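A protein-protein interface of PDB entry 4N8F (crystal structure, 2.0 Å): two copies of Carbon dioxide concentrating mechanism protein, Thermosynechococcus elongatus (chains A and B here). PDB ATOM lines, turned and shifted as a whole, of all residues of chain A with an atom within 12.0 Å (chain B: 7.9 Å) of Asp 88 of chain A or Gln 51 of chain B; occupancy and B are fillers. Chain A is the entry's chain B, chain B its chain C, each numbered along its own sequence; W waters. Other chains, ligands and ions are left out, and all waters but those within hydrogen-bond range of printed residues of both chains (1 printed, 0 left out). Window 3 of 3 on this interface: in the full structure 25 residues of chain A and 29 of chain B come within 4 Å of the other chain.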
ATOM      1  N   ILE A   3       0.185 -28.861  12.687  1.00  0.00           N
ATOM      2  CA  ILE A   3       0.871 -30.175  12.627  1.00  0.00           C
ATOM      3  C   ILE A   3      -0.034 -31.185  11.943  1.00  0.00           C
ATOM      4  O   ILE A   3      -1.207 -31.246  12.253  1.00  0.00           O
ATOM      5  CB  ILE A   3       1.267 -30.642  14.043  1.00  0.00           C
ATOM      6  CG1 ILE A   3       2.243 -29.636  14.667  1.00  0.00           C
ATOM      7  CG2 ILE A   3       1.962 -32.007  13.988  1.00  0.00           C
ATOM      8  CD1 ILE A   3       2.444 -29.772  16.167  1.00  0.00           C
ATOM      9  N   LEU A  30      -3.368 -33.074  13.190  1.00  0.00           N
ATOM     10  CA  LEU A  30      -3.282 -33.421  14.608  1.00  0.00           C
ATOM     11  C   LEU A  30      -4.308 -32.664  15.431  1.00  0.00           C
ATOM     12  O   LEU A  30      -4.438 -31.453  15.297  1.00  0.00           O
ATOM     13  CB  LEU A  30      -1.895 -33.086  15.149  1.00  0.00           C
ATOM     14  CG  LEU A  30      -1.591 -33.462  16.613  1.00  0.00           C
ATOM     15  CD1 LEU A  30      -1.116 -34.900  16.724  1.00  0.00           C
ATOM     16  CD2 LEU A  30      -0.541 -32.547  17.232  1.00  0.00           C
ATOM     17  N   GLY A  31      -5.031 -33.391  16.274  1.00  0.00           N
ATOM     18  CA  GLY A  31      -5.838 -32.791  17.332  1.00  0.00           C
ATOM     19  C   GLY A  31      -5.040 -32.592  18.627  1.00  0.00           C
ATOM     20  O   GLY A  31      -3.878 -32.174  18.611  1.00  0.00           O
ATOM     21  N   GLU A  32      -5.670 -32.856  19.766  1.00  0.00           N
ATOM     22  CA  GLU A  32      -5.005 -32.621  21.048  1.00  0.00           C
ATOM     23  C   GLU A  32      -4.936 -33.972  21.733  1.00  0.00           C
ATOM     24  O   GLU A  32      -5.505 -34.966  21.249  1.00  0.00           O
ATOM     25  CB  GLU A  32      -5.636 -31.454  21.873  1.00  0.00           C
ATOM     26  CG  GLU A  32      -5.242 -30.030  21.357  1.00  0.00           C
ATOM     27  CD  GLU A  32      -4.762 -29.038  22.448  1.00  0.00           C
ATOM     28  OE1 GLU A  32      -5.009 -29.304  23.652  1.00  0.00           O
ATOM     29  OE2 GLU A  32      -4.122 -27.980  22.126  1.00  0.00           O
ATOM     30  N   ASP A  33      -4.175 -34.014  22.817  1.00  0.00           N
ATOM     31  CA  ASP A  33      -3.332 -35.162  23.077  1.00  0.00           C
ATOM     32  C   ASP A  33      -2.487 -35.267  21.788  1.00  0.00           C
ATOM     33  O   ASP A  33      -2.377 -34.288  21.009  1.00  0.00           O
ATOM     34  CB  ASP A  33      -4.144 -36.440  23.356  1.00  0.00           C
ATOM     35  CG  ASP A  33      -4.961 -36.368  24.660  1.00  0.00           C
ATOM     36  OD1 ASP A  33      -6.151 -35.981  24.605  1.00  0.00           O
ATOM     37  OD2 ASP A  33      -4.427 -36.718  25.736  1.00  0.00           O
ATOM     38  N   GLY A  34      -1.888 -36.429  21.546  1.00  0.00           N
ATOM     39  CA  GLY A  34      -1.227 -36.678  20.271  1.00  0.00           C
ATOM     40  C   GLY A  34      -2.132 -37.454  19.331  1.00  0.00           C
ATOM     41  O   GLY A  34      -1.649 -38.324  18.620  1.00  0.00           O
ATOM     42  N   THR A  84      10.936 -33.101  16.087  1.00  0.00           N
ATOM     43  CA  THR A  84      10.452 -33.154  17.441  1.00  0.00           C
ATOM     44  C   THR A  84       9.320 -32.203  17.708  1.00  0.00           C
ATOM     45  O   THR A  84       9.236 -31.119  17.086  1.00  0.00           O
ATOM     46  CB  THR A  84      11.562 -32.855  18.473  1.00  0.00           C
ATOM     47  OG1 THR A  84      11.975 -31.479  18.345  1.00  0.00           O
ATOM     48  CG2 THR A  84      12.745 -33.829  18.323  1.00  0.00           C
ATOM     49  N   VAL A  85       8.447 -32.610  18.628  1.00  0.00           N
ATOM     50  CA  VAL A  85       7.412 -31.714  19.164  1.00  0.00           C
ATOM     51  C   VAL A  85       7.368 -31.872  20.672  1.00  0.00           C
ATOM     52  O   VAL A  85       7.121 -32.975  21.182  1.00  0.00           O
ATOM     53  CB  VAL A  85       6.000 -32.027  18.611  1.00  0.00           C
ATOM     54  CG1 VAL A  85       4.958 -31.112  19.215  1.00  0.00           C
ATOM     55  CG2 VAL A  85       5.972 -31.949  17.108  1.00  0.00           C
ATOM     56  N   SER A  86       7.587 -30.759  21.365  1.00  0.00           N
ATOM     57  CA  SER A  86       7.487 -30.722  22.805  1.00  0.00           C
ATOM     58  C   SER A  86       6.263 -29.945  23.209  1.00  0.00           C
ATOM     59  O   SER A  86       5.823 -29.055  22.464  1.00  0.00           O
ATOM     60  CB  SER A  86       8.725 -30.098  23.383  1.00  0.00           C
ATOM     61  OG  SER A  86       9.837 -30.951  23.115  1.00  0.00           O
ATOM     62  N   ARG A  87       5.722 -30.287  24.376  1.00  0.00           N
ATOM     63  CA  ARG A  87       4.474 -29.709  24.847  1.00  0.00           C
ATOM     64  C   ARG A  87       4.404 -29.729  26.343  1.00  0.00           C
ATOM     65  O   ARG A  87       4.604 -30.741  26.990  1.00  0.00           O
ATOM     66  CB  ARG A  87       3.255 -30.437  24.284  1.00  0.00           C
ATOM     67  CG  ARG A  87       1.914 -29.946  24.818  1.00  0.00           C
ATOM     68  CD  ARG A  87       1.210 -28.963  23.889  1.00  0.00           C
ATOM     69  NE  ARG A  87      -0.150 -28.726  24.394  1.00  0.00           N
ATOM     70  CZ  ARG A  87      -1.147 -28.091  23.757  1.00  0.00           C
ATOM     71  NH1 ARG A  87      -0.993 -27.558  22.552  1.00  0.00           N
ATOM     72  NH2 ARG A  87      -2.331 -27.994  24.344  1.00  0.00           N
ATOM     73  N   ASP A  88       4.095 -28.558  26.859  1.00  0.00           N
ATOM     74  CA  ASP A  88       4.195 -28.209  28.256  1.00  0.00           C
ATOM     75  C   ASP A  88       5.616 -28.382  28.851  1.00  0.00           C
ATOM     76  O   ASP A  88       5.973 -27.641  29.773  1.00  0.00           O
ATOM     77  CB  ASP A  88       3.048 -28.866  29.081  1.00  0.00           C
ATOM     78  CG  ASP A  88       1.735 -28.012  29.091  1.00  0.00           C
ATOM     79  OD1 ASP A  88       1.450 -27.248  28.141  1.00  0.00           O
ATOM     80  OD2 ASP A  88       0.975 -28.101  30.078  1.00  0.00           O
ATOM     81  N   ASN A  89       6.440 -29.296  28.315  1.00  0.00           N
ATOM     82  CA  ASN A  89       7.746 -29.659  28.927  1.00  0.00           C
ATOM     83  C   ASN A  89       8.260 -31.028  28.489  1.00  0.00           C
ATOM     84  O   ASN A  89       9.474 -31.271  28.505  1.00  0.00           O
ATOM     85  CB  ASN A  89       7.662 -29.687  30.450  1.00  0.00           C
ATOM     86  CG  ASN A  89       6.402 -30.387  30.953  1.00  0.00           C
ATOM     87  OD1 ASN A  89       5.380 -30.487  30.248  1.00  0.00           O
ATOM     88  ND2 ASN A  89       6.462 -30.869  32.182  1.00  0.00           N
ATOM     89  N   TYR A  90       7.330 -31.927  28.150  1.00  0.00           N
ATOM     90  CA  TYR A  90       7.664 -33.274  27.691  1.00  0.00           C
ATOM     91  C   TYR A  90       7.598 -33.407  26.167  1.00  0.00           C
ATOM     92  O   TYR A  90       6.998 -32.587  25.451  1.00  0.00           O
ATOM     93  CB  TYR A  90       6.778 -34.340  28.360  1.00  0.00           C
ATOM     94  CG  TYR A  90       5.367 -34.397  27.828  1.00  0.00           C
ATOM     95  CD1 TYR A  90       4.390 -33.513  28.306  1.00  0.00           C
ATOM     96  CD2 TYR A  90       4.998 -35.331  26.851  1.00  0.00           C
ATOM     97  CE1 TYR A  90       3.091 -33.543  27.826  1.00  0.00           C
ATOM     98  CE2 TYR A  90       3.697 -35.373  26.363  1.00  0.00           C
ATOM     99  CZ  TYR A  90       2.742 -34.476  26.857  1.00  0.00           C
ATOM    100  OH  TYR A  90       1.438 -34.490  26.392  1.00  0.00           O
ATOM    101  N   LEU A  91       8.223 -34.481  25.704  1.00  0.00           N
ATOM    102  CA  LEU A  91       8.426 -34.743  24.308  1.00  0.00           C
ATOM    103  C   LEU A  91       7.259 -35.531  23.738  1.00  0.00           C
ATOM    104  O   LEU A  91       7.166 -36.727  23.893  1.00  0.00           O
ATOM    105  CB  LEU A  91       9.722 -35.511  24.161  1.00  0.00           C
ATOM    106  CG  LEU A  91      10.200 -35.800  22.751  1.00  0.00           C
ATOM    107  CD1 LEU A  91      10.782 -34.527  22.187  1.00  0.00           C
ATOM    108  CD2 LEU A  91      11.221 -36.940  22.782  1.00  0.00           C
ATOM    109  N   LEU A  92       6.360 -34.835  23.078  1.00  0.00           N
ATOM    110  CA  LEU A  92       5.166 -35.425  22.499  1.00  0.00           C
ATOM    111  C   LEU A  92       5.527 -36.247  21.270  1.00  0.00           C
ATOM    112  O   LEU A  92       4.930 -37.292  21.020  1.00  0.00           O
ATOM    113  CB  LEU A  92       4.207 -34.282  22.130  1.00  0.00           C
ATOM    114  CG  LEU A  92       2.771 -34.507  21.639  1.00  0.00           C
ATOM    115  CD1 LEU A  92       1.804 -33.525  22.311  1.00  0.00           C
ATOM    116  CD2 LEU A  92       2.697 -34.356  20.133  1.00  0.00           C
ATOM    117  N   TYR A  93       6.504 -35.784  20.491  1.00  0.00           N
ATOM    118  CA  TYR A  93       6.909 -36.527  19.306  1.00  0.00           C
ATOM    119  C   TYR A  93       8.385 -36.424  18.974  1.00  0.00           C
ATOM    120  O   TYR A  93       8.997 -35.397  19.157  1.00  0.00           O
ATOM    121  CB  TYR A  93       6.110 -36.065  18.102  1.00  0.00           C
ATOM    122  CG  TYR A  93       6.543 -36.648  16.773  1.00  0.00           C
ATOM    123  CD1 TYR A  93       7.572 -36.063  16.045  1.00  0.00           C
ATOM    124  CD2 TYR A  93       5.922 -37.787  16.243  1.00  0.00           C
ATOM    125  CE1 TYR A  93       7.960 -36.563  14.826  1.00  0.00           C
ATOM    126  CE2 TYR A  93       6.320 -38.313  15.023  1.00  0.00           C
ATOM    127  CZ  TYR A  93       7.331 -37.675  14.328  1.00  0.00           C
ATOM    128  OH  TYR A  93       7.737 -38.136  13.139  1.00  0.00           O
ATOM    129  N   ARG B   5      -1.184 -18.999  24.825  1.00  0.00           N
ATOM    130  CA  ARG B   5      -0.041 -19.149  25.635  1.00  0.00           C
ATOM    131  C   ARG B   5       0.987 -20.026  24.946  1.00  0.00           C
ATOM    132  O   ARG B   5       0.630 -20.989  24.272  1.00  0.00           O
ATOM    133  CB  ARG B   5      -0.421 -19.699  27.018  1.00  0.00           C
ATOM    134  CG  ARG B   5      -1.083 -21.066  27.060  1.00  0.00           C
ATOM    135  CD  ARG B   5      -0.895 -21.596  28.500  1.00  0.00           C
ATOM    136  NE  ARG B   5      -0.945 -22.975  28.357  1.00  0.00           N
ATOM    137  CZ  ARG B   5       0.020 -23.865  28.448  1.00  0.00           C
ATOM    138  NH1 ARG B   5       1.232 -23.697  29.000  1.00  0.00           N
ATOM    139  NH2 ARG B   5      -0.379 -25.035  28.056  1.00  0.00           N
ATOM    140  N   VAL B   6       2.259 -19.748  25.215  1.00  0.00           N
ATOM    141  CA  VAL B   6       3.316 -20.542  24.625  1.00  0.00           C
ATOM    142  C   VAL B   6       3.399 -21.795  25.363  1.00  0.00           C
ATOM    143  O   VAL B   6       3.496 -21.779  26.558  1.00  0.00           O
ATOM    144  CB  VAL B   6       4.660 -19.871  24.780  1.00  0.00           C
ATOM    145  CG1 VAL B   6       5.763 -20.746  24.223  1.00  0.00           C
ATOM    146  CG2 VAL B   6       4.581 -18.521  24.134  1.00  0.00           C
ATOM    147  N   CYS B   7       3.362 -22.920  24.686  1.00  0.00           N
ATOM    148  CA  CYS B   7       3.370 -24.128  25.465  1.00  0.00           C
ATOM    149  C   CYS B   7       4.307 -25.150  25.002  1.00  0.00           C
ATOM    150  O   CYS B   7       4.384 -26.156  25.665  1.00  0.00           O
ATOM    151  CB  CYS B   7       1.986 -24.742  25.576  1.00  0.00           C
ATOM    152  SG  CYS B   7       1.365 -25.389  24.038  1.00  0.00           S
ATOM    153  N   GLY B   8       5.076 -24.907  23.937  1.00  0.00           N
ATOM    154  CA  GLY B   8       6.113 -25.855  23.548  1.00  0.00           C
ATOM    155  C   GLY B   8       6.856 -25.397  22.323  1.00  0.00           C
ATOM    156  O   GLY B   8       6.859 -24.255  22.044  1.00  0.00           O
ATOM    157  N   THR B   9       7.515 -26.298  21.629  1.00  0.00           N
ATOM    158  CA  THR B   9       8.262 -25.952  20.454  1.00  0.00           C
ATOM    159  C   THR B   9       8.252 -27.114  19.458  1.00  0.00           C
ATOM    160  O   THR B   9       8.066 -28.282  19.849  1.00  0.00           O
ATOM    161  CB  THR B   9       9.755 -25.741  20.764  1.00  0.00           C
ATOM    162  OG1 THR B   9      10.292 -26.989  21.152  1.00  0.00           O
ATOM    163  CG2 THR B   9       9.962 -24.809  21.884  1.00  0.00           C
ATOM    164  N   LYS B  23      12.512 -19.889  14.663  1.00  0.00           N
ATOM    165  CA  LYS B  23      11.969 -20.555  15.820  1.00  0.00           C
ATOM    166  C   LYS B  23      10.480 -20.851  15.709  1.00  0.00           C
ATOM    167  O   LYS B  23       9.673 -19.957  15.497  1.00  0.00           O
ATOM    168  CB  LYS B  23      12.255 -19.777  17.107  1.00  0.00           C
ATOM    169  CG  LYS B  23      12.379 -20.749  18.285  1.00  0.00           C
ATOM    170  CD  LYS B  23      12.018 -20.116  19.620  1.00  0.00           C
ATOM    171  CE  LYS B  23      11.864 -21.187  20.697  1.00  0.00           C
ATOM    172  NZ  LYS B  23      12.969 -22.160  20.722  1.00  0.00           N
ATOM    173  N   LEU B  25       7.223 -22.015  17.747  1.00  0.00           N
ATOM    174  CA  LEU B  25       6.644 -22.268  19.047  1.00  0.00           C
ATOM    175  C   LEU B  25       5.356 -22.980  18.834  1.00  0.00           C
ATOM    176  O   LEU B  25       4.686 -22.719  17.862  1.00  0.00           O
ATOM    177  CB  LEU B  25       6.424 -20.947  19.792  1.00  0.00           C
ATOM    178  CG  LEU B  25       7.652 -20.173  20.271  1.00  0.00           C
ATOM    179  CD1 LEU B  25       7.176 -18.911  20.972  1.00  0.00           C
ATOM    180  CD2 LEU B  25       8.521 -20.987  21.209  1.00  0.00           C
ATOM    181  N   VAL B  26       5.004 -23.878  19.753  1.00  0.00           N
ATOM    182  CA  VAL B  26       3.635 -24.323  19.880  1.00  0.00           C
ATOM    183  C   VAL B  26       2.835 -23.403  20.820  1.00  0.00           C
ATOM    184  O   VAL B  26       3.277 -23.099  21.919  1.00  0.00           O
ATOM    185  CB  VAL B  26       3.580 -25.750  20.397  1.00  0.00           C
ATOM    186  CG1 VAL B  26       2.157 -26.269  20.359  1.00  0.00           C
ATOM    187  CG2 VAL B  26       4.527 -26.649  19.610  1.00  0.00           C
ATOM    188  N   GLN B  28      -1.045 -22.677  22.646  1.00  0.00           N
ATOM    189  CA  GLN B  28      -2.358 -23.132  22.969  1.00  0.00           C
ATOM    190  C   GLN B  28      -3.221 -21.870  23.058  1.00  0.00           C
ATOM    191  O   GLN B  28      -2.902 -20.961  23.785  1.00  0.00           O
ATOM    192  CB  GLN B  28      -2.379 -23.839  24.301  1.00  0.00           C
ATOM    193  CG  GLN B  28      -3.792 -24.321  24.684  1.00  0.00           C
ATOM    194  CD  GLN B  28      -3.786 -25.232  25.890  1.00  0.00           C
ATOM    195  OE1 GLN B  28      -2.870 -25.186  26.708  1.00  0.00           O
ATOM    196  NE2 GLN B  28      -4.817 -26.061  26.012  1.00  0.00           N
ATOM    197  N   PHE B  36      -7.992 -22.755  28.937  1.00  0.00           N
ATOM    198  CA  PHE B  36      -7.047 -23.468  28.085  1.00  0.00           C
ATOM    199  C   PHE B  36      -7.826 -24.239  27.049  1.00  0.00           C
ATOM    200  O   PHE B  36      -8.470 -25.199  27.362  1.00  0.00           O
ATOM    201  CB  PHE B  36      -6.145 -24.405  28.910  1.00  0.00           C
ATOM    202  CG  PHE B  36      -5.040 -23.699  29.680  1.00  0.00           C
ATOM    203  CD1 PHE B  36      -5.186 -22.388  30.099  1.00  0.00           C
ATOM    204  CD2 PHE B  36      -3.871 -24.405  30.052  1.00  0.00           C
ATOM    205  CE1 PHE B  36      -4.171 -21.763  30.828  1.00  0.00           C
ATOM    206  CE2 PHE B  36      -2.873 -23.799  30.796  1.00  0.00           C
ATOM    207  CZ  PHE B  36      -3.019 -22.463  31.177  1.00  0.00           C
ATOM    208  N   GLY B  48      10.692 -13.250  20.814  1.00  0.00           N
ATOM    209  CA  GLY B  48      11.488 -13.798  21.937  1.00  0.00           C
ATOM    210  C   GLY B  48      10.551 -14.193  23.076  1.00  0.00           C
ATOM    211  O   GLY B  48      10.806 -13.872  24.221  1.00  0.00           O
ATOM    212  N   ALA B  49       9.444 -14.877  22.782  1.00  0.00           N
ATOM    213  CA  ALA B  49       8.491 -15.266  23.816  1.00  0.00           C
ATOM    214  C   ALA B  49       8.884 -16.555  24.544  1.00  0.00           C
ATOM    215  O   ALA B  49       9.061 -17.559  23.921  1.00  0.00           O
ATOM    216  CB  ALA B  49       7.099 -15.432  23.226  1.00  0.00           C
ATOM    217  N   GLY B  50       8.946 -16.519  25.873  1.00  0.00           N
ATOM    218  CA  GLY B  50       9.281 -17.693  26.695  1.00  0.00           C
ATOM    219  C   GLY B  50       8.087 -18.600  26.965  1.00  0.00           C
ATOM    220  O   GLY B  50       6.927 -18.240  26.780  1.00  0.00           O
ATOM    221  N   GLN B  51       8.404 -19.786  27.428  1.00  0.00           N
ATOM    222  CA  GLN B  51       7.409 -20.733  27.816  1.00  0.00           C
ATOM    223  C   GLN B  51       6.382 -20.161  28.838  1.00  0.00           C
ATOM    224  O   GLN B  51       6.759 -19.468  29.765  1.00  0.00           O
ATOM    225  CB  GLN B  51       8.111 -21.936  28.384  1.00  0.00           C
ATOM    226  CG  GLN B  51       7.163 -23.044  28.775  1.00  0.00           C
ATOM    227  CD  GLN B  51       6.719 -23.909  27.586  1.00  0.00           C
ATOM    228  OE1 GLN B  51       7.035 -23.628  26.415  1.00  0.00           O
ATOM    229  NE2 GLN B  51       5.971 -24.958  27.894  1.00  0.00           N
ATOM    230  N   ASP B  52       5.110 -20.519  28.657  1.00  0.00           N
ATOM    231  CA  ASP B  52       3.988 -20.056  29.449  1.00  0.00           C
ATOM    232  C   ASP B  52       3.575 -18.593  29.311  1.00  0.00           C
ATOM    233  O   ASP B  52       2.511 -18.237  29.855  1.00  0.00           O
ATOM    234  CB  ASP B  52       4.124 -20.446  30.930  1.00  0.00           C
ATOM    235  CG  ASP B  52       4.070 -21.975  31.134  1.00  0.00           C
ATOM    236  OD1 ASP B  52       3.333 -22.663  30.407  1.00  0.00           O
ATOM    237  OD2 ASP B  52       4.778 -22.486  31.998  1.00  0.00           O
ATOM    238  N   GLU B  53       4.341 -17.767  28.586  1.00  0.00           N
ATOM    239  CA  GLU B  53       3.927 -16.351  28.327  1.00  0.00           C
ATOM    240  C   GLU B  53       2.647 -16.251  27.499  1.00  0.00           C
ATOM    241  O   GLU B  53       2.361 -17.120  26.676  1.00  0.00           O
ATOM    242  CB  GLU B  53       5.018 -15.555  27.651  1.00  0.00           C
ATOM    243  CG  GLU B  53       6.335 -15.665  28.413  1.00  0.00           C
ATOM    244  CD  GLU B  53       7.256 -14.466  28.345  1.00  0.00           C
ATOM    245  OE1 GLU B  53       7.996 -14.249  27.322  1.00  0.00           O
ATOM    246  OE2 GLU B  53       7.319 -13.790  29.392  1.00  0.00           O
ATOM    247  N   TRP B  54       1.831 -15.248  27.806  1.00  0.00           N
ATOM    248  CA  TRP B  54       0.706 -14.961  26.978  1.00  0.00           C
ATOM    249  C   TRP B  54       1.207 -14.136  25.832  1.00  0.00           C
ATOM    250  O   TRP B  54       2.075 -13.239  26.015  1.00  0.00           O
ATOM    251  CB  TRP B  54      -0.407 -14.223  27.739  1.00  0.00           C
ATOM    252  CG  TRP B  54      -1.057 -15.058  28.784  1.00  0.00           C
ATOM    253  CD1 TRP B  54      -0.518 -16.142  29.435  1.00  0.00           C
ATOM    254  CD2 TRP B  54      -2.371 -14.878  29.319  1.00  0.00           C
ATOM    255  NE1 TRP B  54      -1.455 -16.678  30.301  1.00  0.00           N
ATOM    256  CE2 TRP B  54      -2.575 -15.891  30.285  1.00  0.00           C
ATOM    257  CE3 TRP B  54      -3.399 -13.983  29.051  1.00  0.00           C
ATOM    258  CZ2 TRP B  54      -3.767 -16.021  30.996  1.00  0.00           C
ATOM    259  CZ3 TRP B  54      -4.563 -14.084  29.763  1.00  0.00           C
ATOM    260  CH2 TRP B  54      -4.743 -15.094  30.731  1.00  0.00           C
HETATM  261  O   HOH W   1      10.383 -30.153  20.106  1.00  0.00           O
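O of Thr 9 of chain B sits at hydrogen-bond distance from N of Ser 86 of chain A, at 2.9 Å. SG of Cys 7 of chain B lies within hydrogen-bond range of NH1 of Arg 87 of chain A. OD1 of Asp 88 of chain A lies within salt-bridge range of NH2 of Arg 5 of chain B (2.9 Å). The backbone carbonyl oxygen (O) of Cys 7 of chain B sits at hydrogen-bond distance from the backbone NH (N) of Asp 88 of chain A (2.7 Å). The backbone carbonyl oxygen (O) of Asp 88 of chain A is in hydrogen-bond range of the side-chain amide nitrogen (NE2) of Gln 51 of chain B (3.3 Å).
NH2 of Arg 87 of chain A lies within salt-bridge range of OE2 of Glu 32 of chain A (2.9 Å). The backbone carbonyl oxygen (O) of Val 85 of chain A sits at hydrogen-bond distance from the backbone NH (N) of Leu 92 of chain A, 2.8 Å away. The backbone carbonyl oxygen of Arg 87 of chain A lies close to the side-chain amide oxygen of Asn 89 of chain A, at 3.4 Å. O of Gln 28 of chain B lies within hydrogen-bond range of N of Arg 5 of chain B, 2.8 Å away. O of Cys 7 of chain B sits at hydrogen-bond distance from NE2 of Gln 51 of chain B. The backbone NH of Gly 8 of chain B sits at hydrogen-bond distance from the side-chain amide oxygen of Gln 51 of chain B (3.4 Å).
Among the printed residues, pairs that only touch across the chains: Val 85 of chain A with Thr 9 of chain B (3.6 Å), Ser 86 of chain A with Gly 8 of chain B (3.4 Å), Ser 86 of chain A with Val 26 of chain B (3.95 Å) and Arg 87 of chain A with Gln 28 of chain B (3.5 Å).
Ile 3 of chain A touches none of the printed residues of chain B. Printed residues of chain B within 4 Å of Asp 88 of chain A: Arg 5, Cys 7 and Gln 51. Tyr 93 of chain A touches none of the printed residues of chain B. Printed residues of chain A within 4 Å of Arg 5 of chain B: Asp 88. No residue of chain A comes within 4 Å of Val 6 of chain B. Of chain A, only Arg 87 and Asp 88 come within 4 Å of Cys 7 of chain B. Gly 8 of chain B touches just one residue of chain A: Ser 86. Of the printed residues of chain A, Thr 9 of chain B touches Val 85 (3.6 Å) and Ser 86 (2.9 Å). Val 26 of chain B touches just one residue of chain A: Ser 86 (3.95 Å). No residue of chain A comes within 4 Å of Ala 49 of chain B. No residue of chain A comes within 4 Å of Gly 50 of chain B. Gln 51 of chain B touches one residue of chain A. No residue of chain A comes within 4 Å of Asp 52 of chain B. No residue of chain A comes within 4 Å of Glu 53 of chain B. The nearest printed residue of chain A that does not touch Gln 28 of chain B is Glu 32 of chain A (4.02 Å).
Of the 17 printed residues of chain B, 7 touch a printed residue of chain A. Printed residues of chain A that touch a printed residue of chain B: Val 85, Ser 86, Arg 87 and Asp 88. Among the printed residues, 9 pairs touch across the chains. Among the printed residues, Asp or Glu carboxylates within 4 Å of a Lys or Arg side-chain nitrogen of the other chain: Asp 88 of chain A with Arg 5 of chain B (2.9 Å).
No position is printed for both chains. Of the 9 pairs that touch across the chains among the printed residues, none has its exchanged pair printed and touching as well.
Water W1 lies within hydrogen-bond range of the side-chain hydroxyl of Thr 84 of chain A (2.7 Å), the backbone carbonyl oxygen of Thr 9 of chain B (3.0 Å), the backbone NH of Ser 86 of chain A (3.1 Å) and the backbone NH of Val 85 of chain A (3.5 Å).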
